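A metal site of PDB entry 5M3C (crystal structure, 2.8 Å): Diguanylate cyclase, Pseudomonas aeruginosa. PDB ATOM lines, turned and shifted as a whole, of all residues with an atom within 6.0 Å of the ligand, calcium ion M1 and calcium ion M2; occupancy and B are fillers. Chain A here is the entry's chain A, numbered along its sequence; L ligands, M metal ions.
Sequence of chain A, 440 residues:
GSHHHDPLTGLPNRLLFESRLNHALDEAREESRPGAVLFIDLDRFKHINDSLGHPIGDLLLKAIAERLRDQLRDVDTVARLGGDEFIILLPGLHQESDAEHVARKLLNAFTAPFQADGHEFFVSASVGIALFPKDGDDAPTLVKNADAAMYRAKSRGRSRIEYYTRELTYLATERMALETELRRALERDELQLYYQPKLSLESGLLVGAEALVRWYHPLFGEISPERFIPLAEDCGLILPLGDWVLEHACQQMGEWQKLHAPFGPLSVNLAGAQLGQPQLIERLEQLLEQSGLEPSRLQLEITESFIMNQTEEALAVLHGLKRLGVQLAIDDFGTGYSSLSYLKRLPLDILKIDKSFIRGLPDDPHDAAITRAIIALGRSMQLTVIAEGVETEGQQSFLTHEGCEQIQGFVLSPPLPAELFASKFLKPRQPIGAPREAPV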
ATOM      1  N   LEU A   8      15.188  29.177  -4.356  1.00  0.00           N
ATOM      2  CA  LEU A   8      15.403  27.910  -3.683  1.00  0.00           C
ATOM      3  C   LEU A   8      14.388  26.845  -4.087  1.00  0.00           C
ATOM      4  O   LEU A   8      14.748  25.702  -4.393  1.00  0.00           O
ATOM      5  CB  LEU A   8      15.379  28.101  -2.167  1.00  0.00           C
ATOM      6  CG  LEU A   8      15.355  26.828  -1.308  1.00  0.00           C
ATOM      7  CD1 LEU A   8      16.466  25.862  -1.700  1.00  0.00           C
ATOM      8  CD2 LEU A   8      15.450  27.193   0.165  1.00  0.00           C
ATOM      9  N   ASP A  41       2.736  26.678   7.979  1.00  0.00           N
ATOM     10  CA  ASP A  41       4.011  26.926   8.636  1.00  0.00           C
ATOM     11  C   ASP A  41       4.514  25.612   9.220  1.00  0.00           C
ATOM     12  O   ASP A  41       3.746  24.856   9.818  1.00  0.00           O
ATOM     13  CB  ASP A  41       3.838  27.981   9.738  1.00  0.00           C
ATOM     14  CG  ASP A  41       5.106  28.212  10.522  1.00  0.00           C
ATOM     15  OD1 ASP A  41       5.492  27.333  11.312  1.00  0.00           O
ATOM     16  OD2 ASP A  41       5.708  29.291  10.365  1.00  0.00           O
ATOM     17  N   LEU A  42       5.798  25.338   9.045  1.00  0.00           N
ATOM     18  CA  LEU A  42       6.373  24.067   9.442  1.00  0.00           C
ATOM     19  C   LEU A  42       6.538  23.952  10.950  1.00  0.00           C
ATOM     20  O   LEU A  42       6.853  24.930  11.631  1.00  0.00           O
ATOM     21  CB  LEU A  42       7.733  23.847   8.752  1.00  0.00           C
ATOM     22  CG  LEU A  42       7.709  23.860   7.223  1.00  0.00           C
ATOM     23  CD1 LEU A  42       9.126  23.849   6.679  1.00  0.00           C
ATOM     24  CD2 LEU A  42       6.913  22.690   6.664  1.00  0.00           C
ATOM     25  N   ASP A  43       6.319  22.744  11.478  1.00  0.00           N
ATOM     26  CA  ASP A  43       6.404  22.497  12.912  1.00  0.00           C
ATOM     27  C   ASP A  43       7.849  22.345  13.371  1.00  0.00           C
ATOM     28  O   ASP A  43       8.587  21.501  12.870  1.00  0.00           O
ATOM     29  CB  ASP A  43       5.595  21.255  13.291  1.00  0.00           C
ATOM     30  CG  ASP A  43       4.094  21.500  13.276  1.00  0.00           C
ATOM     31  OD1 ASP A  43       3.676  22.669  13.222  1.00  0.00           O
ATOM     32  OD2 ASP A  43       3.327  20.510  13.328  1.00  0.00           O
ATOM     33  N   ARG A  44       8.222  23.179  14.334  1.00  0.00           N
ATOM     34  CA  ARG A  44       9.559  23.166  14.939  1.00  0.00           C
ATOM     35  C   ARG A  44      10.676  22.907  13.926  1.00  0.00           C
ATOM     36  O   ARG A  44      11.255  21.826  13.893  1.00  0.00           O
ATOM     37  CB  ARG A  44       9.597  22.139  16.076  1.00  0.00           C
ATOM     38  CG  ARG A  44       8.719  22.524  17.250  1.00  0.00           C
ATOM     39  CD  ARG A  44       8.367  21.325  18.127  1.00  0.00           C
ATOM     40  N   PHE A  45      10.968  23.930  13.122  1.00  0.00           N
ATOM     41  CA  PHE A  45      11.964  23.816  12.055  1.00  0.00           C
ATOM     42  C   PHE A  45      13.361  24.287  12.491  1.00  0.00           C
ATOM     43  O   PHE A  45      14.355  23.833  11.926  1.00  0.00           O
ATOM     44  CB  PHE A  45      11.512  24.595  10.826  1.00  0.00           C
ATOM     45  CG  PHE A  45      12.071  24.067   9.539  1.00  0.00           C
ATOM     46  CD1 PHE A  45      11.785  22.774   9.135  1.00  0.00           C
ATOM     47  CD2 PHE A  45      12.885  24.846   8.735  1.00  0.00           C
ATOM     48  CE1 PHE A  45      12.292  22.266   7.963  1.00  0.00           C
ATOM     49  CE2 PHE A  45      13.400  24.344   7.552  1.00  0.00           C
ATOM     50  CZ  PHE A  45      13.099  23.054   7.167  1.00  0.00           C
ATOM     51  N   LYS A  46      13.424  25.185  13.461  1.00  0.00           N
ATOM     52  CA  LYS A  46      14.727  25.650  13.969  1.00  0.00           C
ATOM     53  C   LYS A  46      15.523  24.468  14.496  1.00  0.00           C
ATOM     54  O   LYS A  46      16.692  24.267  14.131  1.00  0.00           O
ATOM     55  CB  LYS A  46      14.543  26.696  15.069  1.00  0.00           C
ATOM     56  N   HIS A  47      14.886  23.660  15.341  1.00  0.00           N
ATOM     57  CA  HIS A  47      15.500  22.462  15.920  1.00  0.00           C
ATOM     58  C   HIS A  47      16.080  21.559  14.837  1.00  0.00           C
ATOM     59  O   HIS A  47      17.067  20.857  15.069  1.00  0.00           O
ATOM     60  CB  HIS A  47      14.483  21.678  16.742  1.00  0.00           C
ATOM     61  N   ASN A  49      17.084  22.807  11.759  1.00  0.00           N
ATOM     62  CA  ASN A  49      18.199  23.558  11.182  1.00  0.00           C
ATOM     63  C   ASN A  49      19.446  23.452  12.059  1.00  0.00           C
ATOM     64  O   ASN A  49      20.563  23.383  11.549  1.00  0.00           O
ATOM     65  CB  ASN A  49      17.833  25.035  10.995  1.00  0.00           C
ATOM     66  CG  ASN A  49      17.303  25.322   9.604  1.00  0.00           C
ATOM     67  OD1 ASN A  49      16.873  24.421   8.883  1.00  0.00           O
ATOM     68  ND2 ASN A  49      17.324  26.599   9.226  1.00  0.00           N
ATOM     69  N   GLY A  53      21.456  21.053  10.272  1.00  0.00           N
ATOM     70  CA  GLY A  53      22.168  22.061   9.486  1.00  0.00           C
ATOM     71  C   GLY A  53      21.432  22.477   8.225  1.00  0.00           C
ATOM     72  O   GLY A  53      20.676  21.691   7.647  1.00  0.00           O
ATOM     73  N   HIS A  54      21.667  23.707   7.793  1.00  0.00           N
ATOM     74  CA  HIS A  54      21.029  24.260   6.593  1.00  0.00           C
ATOM     75  C   HIS A  54      21.001  23.288   5.405  1.00  0.00           C
ATOM     76  O   HIS A  54      19.970  23.164   4.735  1.00  0.00           O
ATOM     77  CB  HIS A  54      21.720  25.562   6.164  1.00  0.00           C
ATOM     78  CG  HIS A  54      20.908  26.791   6.457  1.00  0.00           C
ATOM     79  ND1 HIS A  54      20.407  27.596   5.468  1.00  0.00           N
ATOM     80  CD2 HIS A  54      20.525  27.337   7.632  1.00  0.00           C
ATOM     81  CE1 HIS A  54      19.741  28.601   6.016  1.00  0.00           C
ATOM     82  NE2 HIS A  54      19.800  28.470   7.324  1.00  0.00           N
ATOM     83  N   PRO A  55      22.133  22.627   5.107  1.00  0.00           N
ATOM     84  CA  PRO A  55      22.165  21.653   4.024  1.00  0.00           C
ATOM     85  C   PRO A  55      20.883  20.828   3.950  1.00  0.00           C
ATOM     86  O   PRO A  55      20.246  20.768   2.903  1.00  0.00           O
ATOM     87  CB  PRO A  55      23.359  20.765   4.395  1.00  0.00           C
ATOM     88  CG  PRO A  55      24.223  21.601   5.293  1.00  0.00           C
ATOM     89  CD  PRO A  55      23.470  22.841   5.688  1.00  0.00           C
ATOM     90  N   ILE A  56      20.522  20.185   5.057  1.00  0.00           N
ATOM     91  CA  ILE A  56      19.321  19.368   5.124  1.00  0.00           C
ATOM     92  C   ILE A  56      18.077  20.238   4.989  1.00  0.00           C
ATOM     93  O   ILE A  56      17.135  19.904   4.255  1.00  0.00           O
ATOM     94  CB  ILE A  56      19.249  18.576   6.445  1.00  0.00           C
ATOM     95  CG1 ILE A  56      20.479  17.682   6.605  1.00  0.00           C
ATOM     96  CG2 ILE A  56      17.973  17.752   6.504  1.00  0.00           C
ATOM     97  CD1 ILE A  56      20.620  16.611   5.538  1.00  0.00           C
ATOM     98  N   GLY A  57      18.066  21.364   5.700  1.00  0.00           N
ATOM     99  CA  GLY A  57      16.949  22.300   5.656  1.00  0.00           C
ATOM    100  C   GLY A  57      16.569  22.705   4.250  1.00  0.00           C
ATOM    101  O   GLY A  57      15.498  22.335   3.762  1.00  0.00           O
ATOM    102  N   ASP A  58      17.443  23.461   3.586  1.00  0.00           N
ATOM    103  CA  ASP A  58      17.179  23.944   2.234  1.00  0.00           C
ATOM    104  C   ASP A  58      16.658  22.842   1.322  1.00  0.00           C
ATOM    105  O   ASP A  58      15.884  23.104   0.401  1.00  0.00           O
ATOM    106  CB  ASP A  58      18.455  24.570   1.628  1.00  0.00           C
ATOM    107  CG  ASP A  58      18.763  25.937   2.196  1.00  0.00           C
ATOM    108  OD1 ASP A  58      18.609  26.121   3.426  1.00  0.00           O
ATOM    109  OD2 ASP A  58      19.172  26.824   1.431  1.00  0.00           O
ATOM    110  N   LEU A  61      12.875  21.785   2.360  1.00  0.00           N
ATOM    111  CA  LEU A  61      11.954  22.780   1.821  1.00  0.00           C
ATOM    112  C   LEU A  61      11.622  22.480   0.359  1.00  0.00           C
ATOM    113  O   LEU A  61      10.464  22.543  -0.043  1.00  0.00           O
ATOM    114  CB  LEU A  61      12.538  24.190   1.959  1.00  0.00           C
ATOM    115  CG  LEU A  61      12.712  24.711   3.388  1.00  0.00           C
ATOM    116  CD1 LEU A  61      13.480  26.020   3.395  1.00  0.00           C
ATOM    117  CD2 LEU A  61      11.375  24.869   4.079  1.00  0.00           C
ATOM    118  N   ARG A  80       5.910  30.224  -1.665  1.00  0.00           N
ATOM    119  CA  ARG A  80       6.697  30.368  -0.446  1.00  0.00           C
ATOM    120  C   ARG A  80       6.690  31.834  -0.080  1.00  0.00           C
ATOM    121  O   ARG A  80       7.045  32.686  -0.890  1.00  0.00           O
ATOM    122  CB  ARG A  80       8.142  29.889  -0.653  1.00  0.00           C
ATOM    123  CG  ARG A  80       8.845  29.493   0.643  1.00  0.00           C
ATOM    124  CD  ARG A  80      10.282  29.029   0.412  1.00  0.00           C
ATOM    125  NE  ARG A  80      11.260  30.078   0.717  1.00  0.00           N
ATOM    126  CZ  ARG A  80      12.154  30.014   1.709  1.00  0.00           C
ATOM    127  NH1 ARG A  80      13.008  31.013   1.895  1.00  0.00           N
ATOM    128  NH2 ARG A  80      12.212  28.958   2.502  1.00  0.00           N
ATOM    129  N   GLY A  82       8.379  33.262   2.281  1.00  0.00           N
ATOM    130  CA  GLY A  82       9.589  33.615   3.013  1.00  0.00           C
ATOM    131  C   GLY A  82       9.641  32.817   4.294  1.00  0.00           C
ATOM    132  O   GLY A  82       8.606  32.505   4.888  1.00  0.00           O
ATOM    133  N   GLY A  83      10.853  32.481   4.724  1.00  0.00           N
ATOM    134  CA  GLY A  83      11.022  31.625   5.898  1.00  0.00           C
ATOM    135  C   GLY A  83      10.491  30.238   5.613  1.00  0.00           C
ATOM    136  O   GLY A  83      10.498  29.773   4.474  1.00  0.00           O
ATOM    137  N   ASP A  84      10.019  29.558   6.654  1.00  0.00           N
ATOM    138  CA  ASP A  84       9.494  28.202   6.510  1.00  0.00           C
ATOM    139  C   ASP A  84       7.982  28.243   6.328  1.00  0.00           C
ATOM    140  O   ASP A  84       7.260  27.473   6.977  1.00  0.00           O
ATOM    141  CB  ASP A  84       9.842  27.362   7.729  1.00  0.00           C
ATOM    142  CG  ASP A  84       9.140  27.837   8.984  1.00  0.00           C
ATOM    143  OD1 ASP A  84       8.661  28.989   9.011  1.00  0.00           O
ATOM    144  OD2 ASP A  84       9.066  27.056   9.957  1.00  0.00           O
ATOM    145  N   GLU A  85       7.500  29.118   5.453  1.00  0.00           N
ATOM    146  CA  GLU A  85       6.077  29.385   5.344  1.00  0.00           C
ATOM    147  C   GLU A  85       5.580  29.345   3.902  1.00  0.00           C
ATOM    148  O   GLU A  85       6.079  30.065   3.039  1.00  0.00           O
ATOM    149  CB  GLU A  85       5.754  30.728   5.989  1.00  0.00           C
ATOM    150  CG  GLU A  85       5.969  30.747   7.498  1.00  0.00           C
ATOM    151  CD  GLU A  85       5.925  32.139   8.109  1.00  0.00           C
ATOM    152  OE1 GLU A  85       5.767  33.125   7.360  1.00  0.00           O
ATOM    153  OE2 GLU A  85       6.045  32.230   9.348  1.00  0.00           O
ATOM    154  N   LYS A 154      -0.938  26.144  16.129  1.00  0.00           N
ATOM    155  CA  LYS A 154       0.211  26.087  17.029  1.00  0.00           C
ATOM    156  C   LYS A 154      -0.286  26.074  18.473  1.00  0.00           C
ATOM    157  O   LYS A 154       0.216  25.323  19.314  1.00  0.00           O
ATOM    158  CB  LYS A 154       1.114  27.305  16.840  1.00  0.00           C
ATOM    159  CG  LYS A 154       1.752  27.409  15.464  1.00  0.00           C
ATOM    160  CD  LYS A 154       2.624  26.198  15.165  1.00  0.00           C
ATOM    161  CE  LYS A 154       3.516  26.462  13.968  1.00  0.00           C
ATOM    162  NZ  LYS A 154       4.063  25.188  13.426  1.00  0.00           N
ATOM    163  N   ARG A 158      -0.062  20.770  17.868  1.00  0.00           N
ATOM    164  CA  ARG A 158       0.519  21.065  16.559  1.00  0.00           C
ATOM    165  C   ARG A 158       0.078  20.037  15.525  1.00  0.00           C
ATOM    166  O   ARG A 158      -0.775  19.191  15.806  1.00  0.00           O
ATOM    167  CB  ARG A 158       2.046  21.114  16.647  1.00  0.00           C
ATOM    168  CG  ARG A 158       2.585  22.474  17.034  1.00  0.00           C
ATOM    169  CD  ARG A 158       4.095  22.460  17.209  1.00  0.00           C
ATOM    170  NE  ARG A 158       4.630  23.784  17.501  1.00  0.00           N
ATOM    171  CZ  ARG A 158       4.418  24.464  18.628  1.00  0.00           C
ATOM    172  NH1 ARG A 158       4.951  25.665  18.792  1.00  0.00           N
ATOM    173  NH2 ARG A 158       3.662  23.947  19.586  1.00  0.00           N
ATOM    174  N   ASP A 234       9.104  28.353  23.307  1.00  0.00           N
ATOM    175  CA  ASP A 234       9.211  29.258  22.160  1.00  0.00           C
ATOM    176  C   ASP A 234      10.237  30.364  22.379  1.00  0.00           C
ATOM    177  O   ASP A 234      11.012  30.690  21.476  1.00  0.00           O
ATOM    178  CB  ASP A 234       7.838  29.859  21.838  1.00  0.00           C
ATOM    179  CG  ASP A 234       6.858  28.812  21.337  1.00  0.00           C
ATOM    180  OD1 ASP A 234       7.269  27.931  20.550  1.00  0.00           O
ATOM    181  OD2 ASP A 234       5.670  28.866  21.734  1.00  0.00           O
HETATM  182  P1  LIG L   1       7.218  26.629  15.464  1.00  0.00           P
HETATM  183  O1  LIG L   1       6.502  25.365  15.876  1.00  0.00           O
HETATM  184  O2  LIG L   1       6.897  27.065  14.048  1.00  0.00           O
HETATM  185  O3  LIG L   1       7.160  27.734  16.493  1.00  0.00           O
HETATM  186  O4  LIG L   1       8.776  26.206  15.408  1.00  0.00           O
HETATM  187  P2  LIG L   1       9.823  26.928  14.428  1.00  0.00           P
HETATM  188  O5  LIG L   1      11.220  26.592  14.891  1.00  0.00           O
HETATM  189  O6  LIG L   1       9.439  26.624  13.003  1.00  0.00           O
HETATM  190  O7  LIG L   1       9.573  28.494  14.708  1.00  0.00           O
HETATM  191  P3  LIG L   1       9.796  29.571  13.542  1.00  0.00           P
HETATM  192  O8  LIG L   1      10.101  30.900  14.172  1.00  0.00           O
HETATM  193  O9  LIG L   1       8.691  29.446  12.524  1.00  0.00           O
HETATM  194  O10 LIG L   1      11.137  29.020  12.876  1.00  0.00           O
HETATM  195  C1  LIG L   1      11.539  29.507  11.607  1.00  0.00           C
HETATM  196  C2  LIG L   1      12.801  28.748  11.246  1.00  0.00           C
HETATM  197  O11 LIG L   1      12.822  28.418   9.861  1.00  0.00           O
HETATM  198  C3  LIG L   1      14.023  29.591  11.557  1.00  0.00           C
HETATM  199  O12 LIG L   1      14.912  28.866  12.415  1.00  0.00           O
HETATM  200  C4  LIG L   1      14.654  29.837  10.201  1.00  0.00           C
HETATM  201  O13 LIG L   1      16.077  29.855  10.250  1.00  0.00           O
HETATM  202  C5  LIG L   1      14.138  28.668   9.380  1.00  0.00           C
HETATM  203  N1  LIG L   1      14.208  29.029   7.952  1.00  0.00           N
HETATM  204  C6  LIG L   1      13.609  30.069   7.339  1.00  0.00           C
HETATM  205  N2  LIG L   1      13.933  30.089   6.022  1.00  0.00           N
HETATM  206  C7  LIG L   1      14.766  29.049   5.783  1.00  0.00           C
HETATM  207  C8  LIG L   1      15.486  28.488   4.626  1.00  0.00           C
HETATM  208  O14 LIG L   1      15.377  29.011   3.501  1.00  0.00           O
HETATM  209  N3  LIG L   1      16.251  27.398   4.815  1.00  0.00           N
HETATM  210  C9  LIG L   1      16.374  26.808   6.028  1.00  0.00           C
HETATM  211  N4  LIG L   1      17.161  25.711   6.145  1.00  0.00           N
HETATM  212  N5  LIG L   1      15.745  27.269   7.131  1.00  0.00           N
HETATM  213  C10 LIG L   1      14.941  28.362   7.064  1.00  0.00           C
HETATM  214 CA    CA M   1       7.837  30.922  10.477  1.00  0.00          CA
HETATM  215 CA    CA M   2       7.578  27.271  11.697  1.00  0.00          CA
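A nitrogen (N5) of the ligand is in hydrogen-bond range of the side-chain amide nitrogen of Asn 49, 2.7 Å away. O1 of the ligand lies within salt-bridge range of NE of Arg 158, 2.9 Å away. O5 of the ligand lies within hydrogen-bond range of N of Lys 46 (3.0 Å). OD1 of Asp 58 lies within hydrogen-bond range of N3 of the ligand (3.0 Å). The backbone NH of Phe 45 sits at hydrogen-bond distance from an oxygen (O5) of the ligand, at 3.2 Å. N of Arg 44 sits at hydrogen-bond distance from O1 of the ligand, 3.2 Å away. O14 of the ligand sits at hydrogen-bond distance from NH2 of Arg 80, at 3.3 Å. An oxygen (O1) of the ligand is in salt-bridge range of the side-chain amino group (NZ) of Lys 154 (3.5 Å).
OD1 of Asp 41 sits close to NZ of Lys 154 (3.3 Å). NZ of Lys 154 sits close to O of Leu 42. The side-chain carboxylate (OD1) of Asp 234 lies within salt-bridge range of the guanidinium group (NH1) of Arg 158. The side-chain carboxylate of Asp 58 lies within hydrogen-bond range of a ring nitrogen (ND1) of His 54 (3.1 Å). O of Gly 83 sits at hydrogen-bond distance from NH2 of Arg 80. NZ of Lys 154 is in salt-bridge range of OD1 of Asp 43 (2.6 Å).
Residues that only touch the ligand: Leu 8, His 54, Gly 57, Leu 61 and Gly 83. Of the 24 residues printed, 16 come within 4 Å of the ligand.
Of the 24 residues printed, 3 come within 4 Å of calcium ion M1. The nearest printed residue that does not touch calcium ion M1 is Gly 83 (5.6 Å).
Along chain A the residues within 4 Å of calcium ion M2 span positions 41 to 84. The nearest printed residue that does not touch calcium ion M2 is Lys 154 (4.4 Å).
Calcium ion M1 is bound by the side-chain carboxylate of Glu 85 (2.5 Å), the side-chain carboxylate of Asp 84 (2.6 Å), an oxygen (O9) of the ligand (2.7 Å) and the side-chain carboxylate of Asp 41 (2.7 Å). Calcium ion M1 has four donor atoms within binding distance.
Calcium ion M2 is bound by OD1 of Asp 41 (2.1 Å), OD2 of Asp 84 (2.3 Å), O6 of the ligand (2.4 Å), O of Leu 42 (2.5 Å), O2 of the ligand (2.5 Å) and O9 of the ligand (2.6 Å). Calcium ion M2 has six donor atoms within binding distance. Slightly farther from calcium ion M2 lies OD2 of Asp 41 (3.1 Å).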
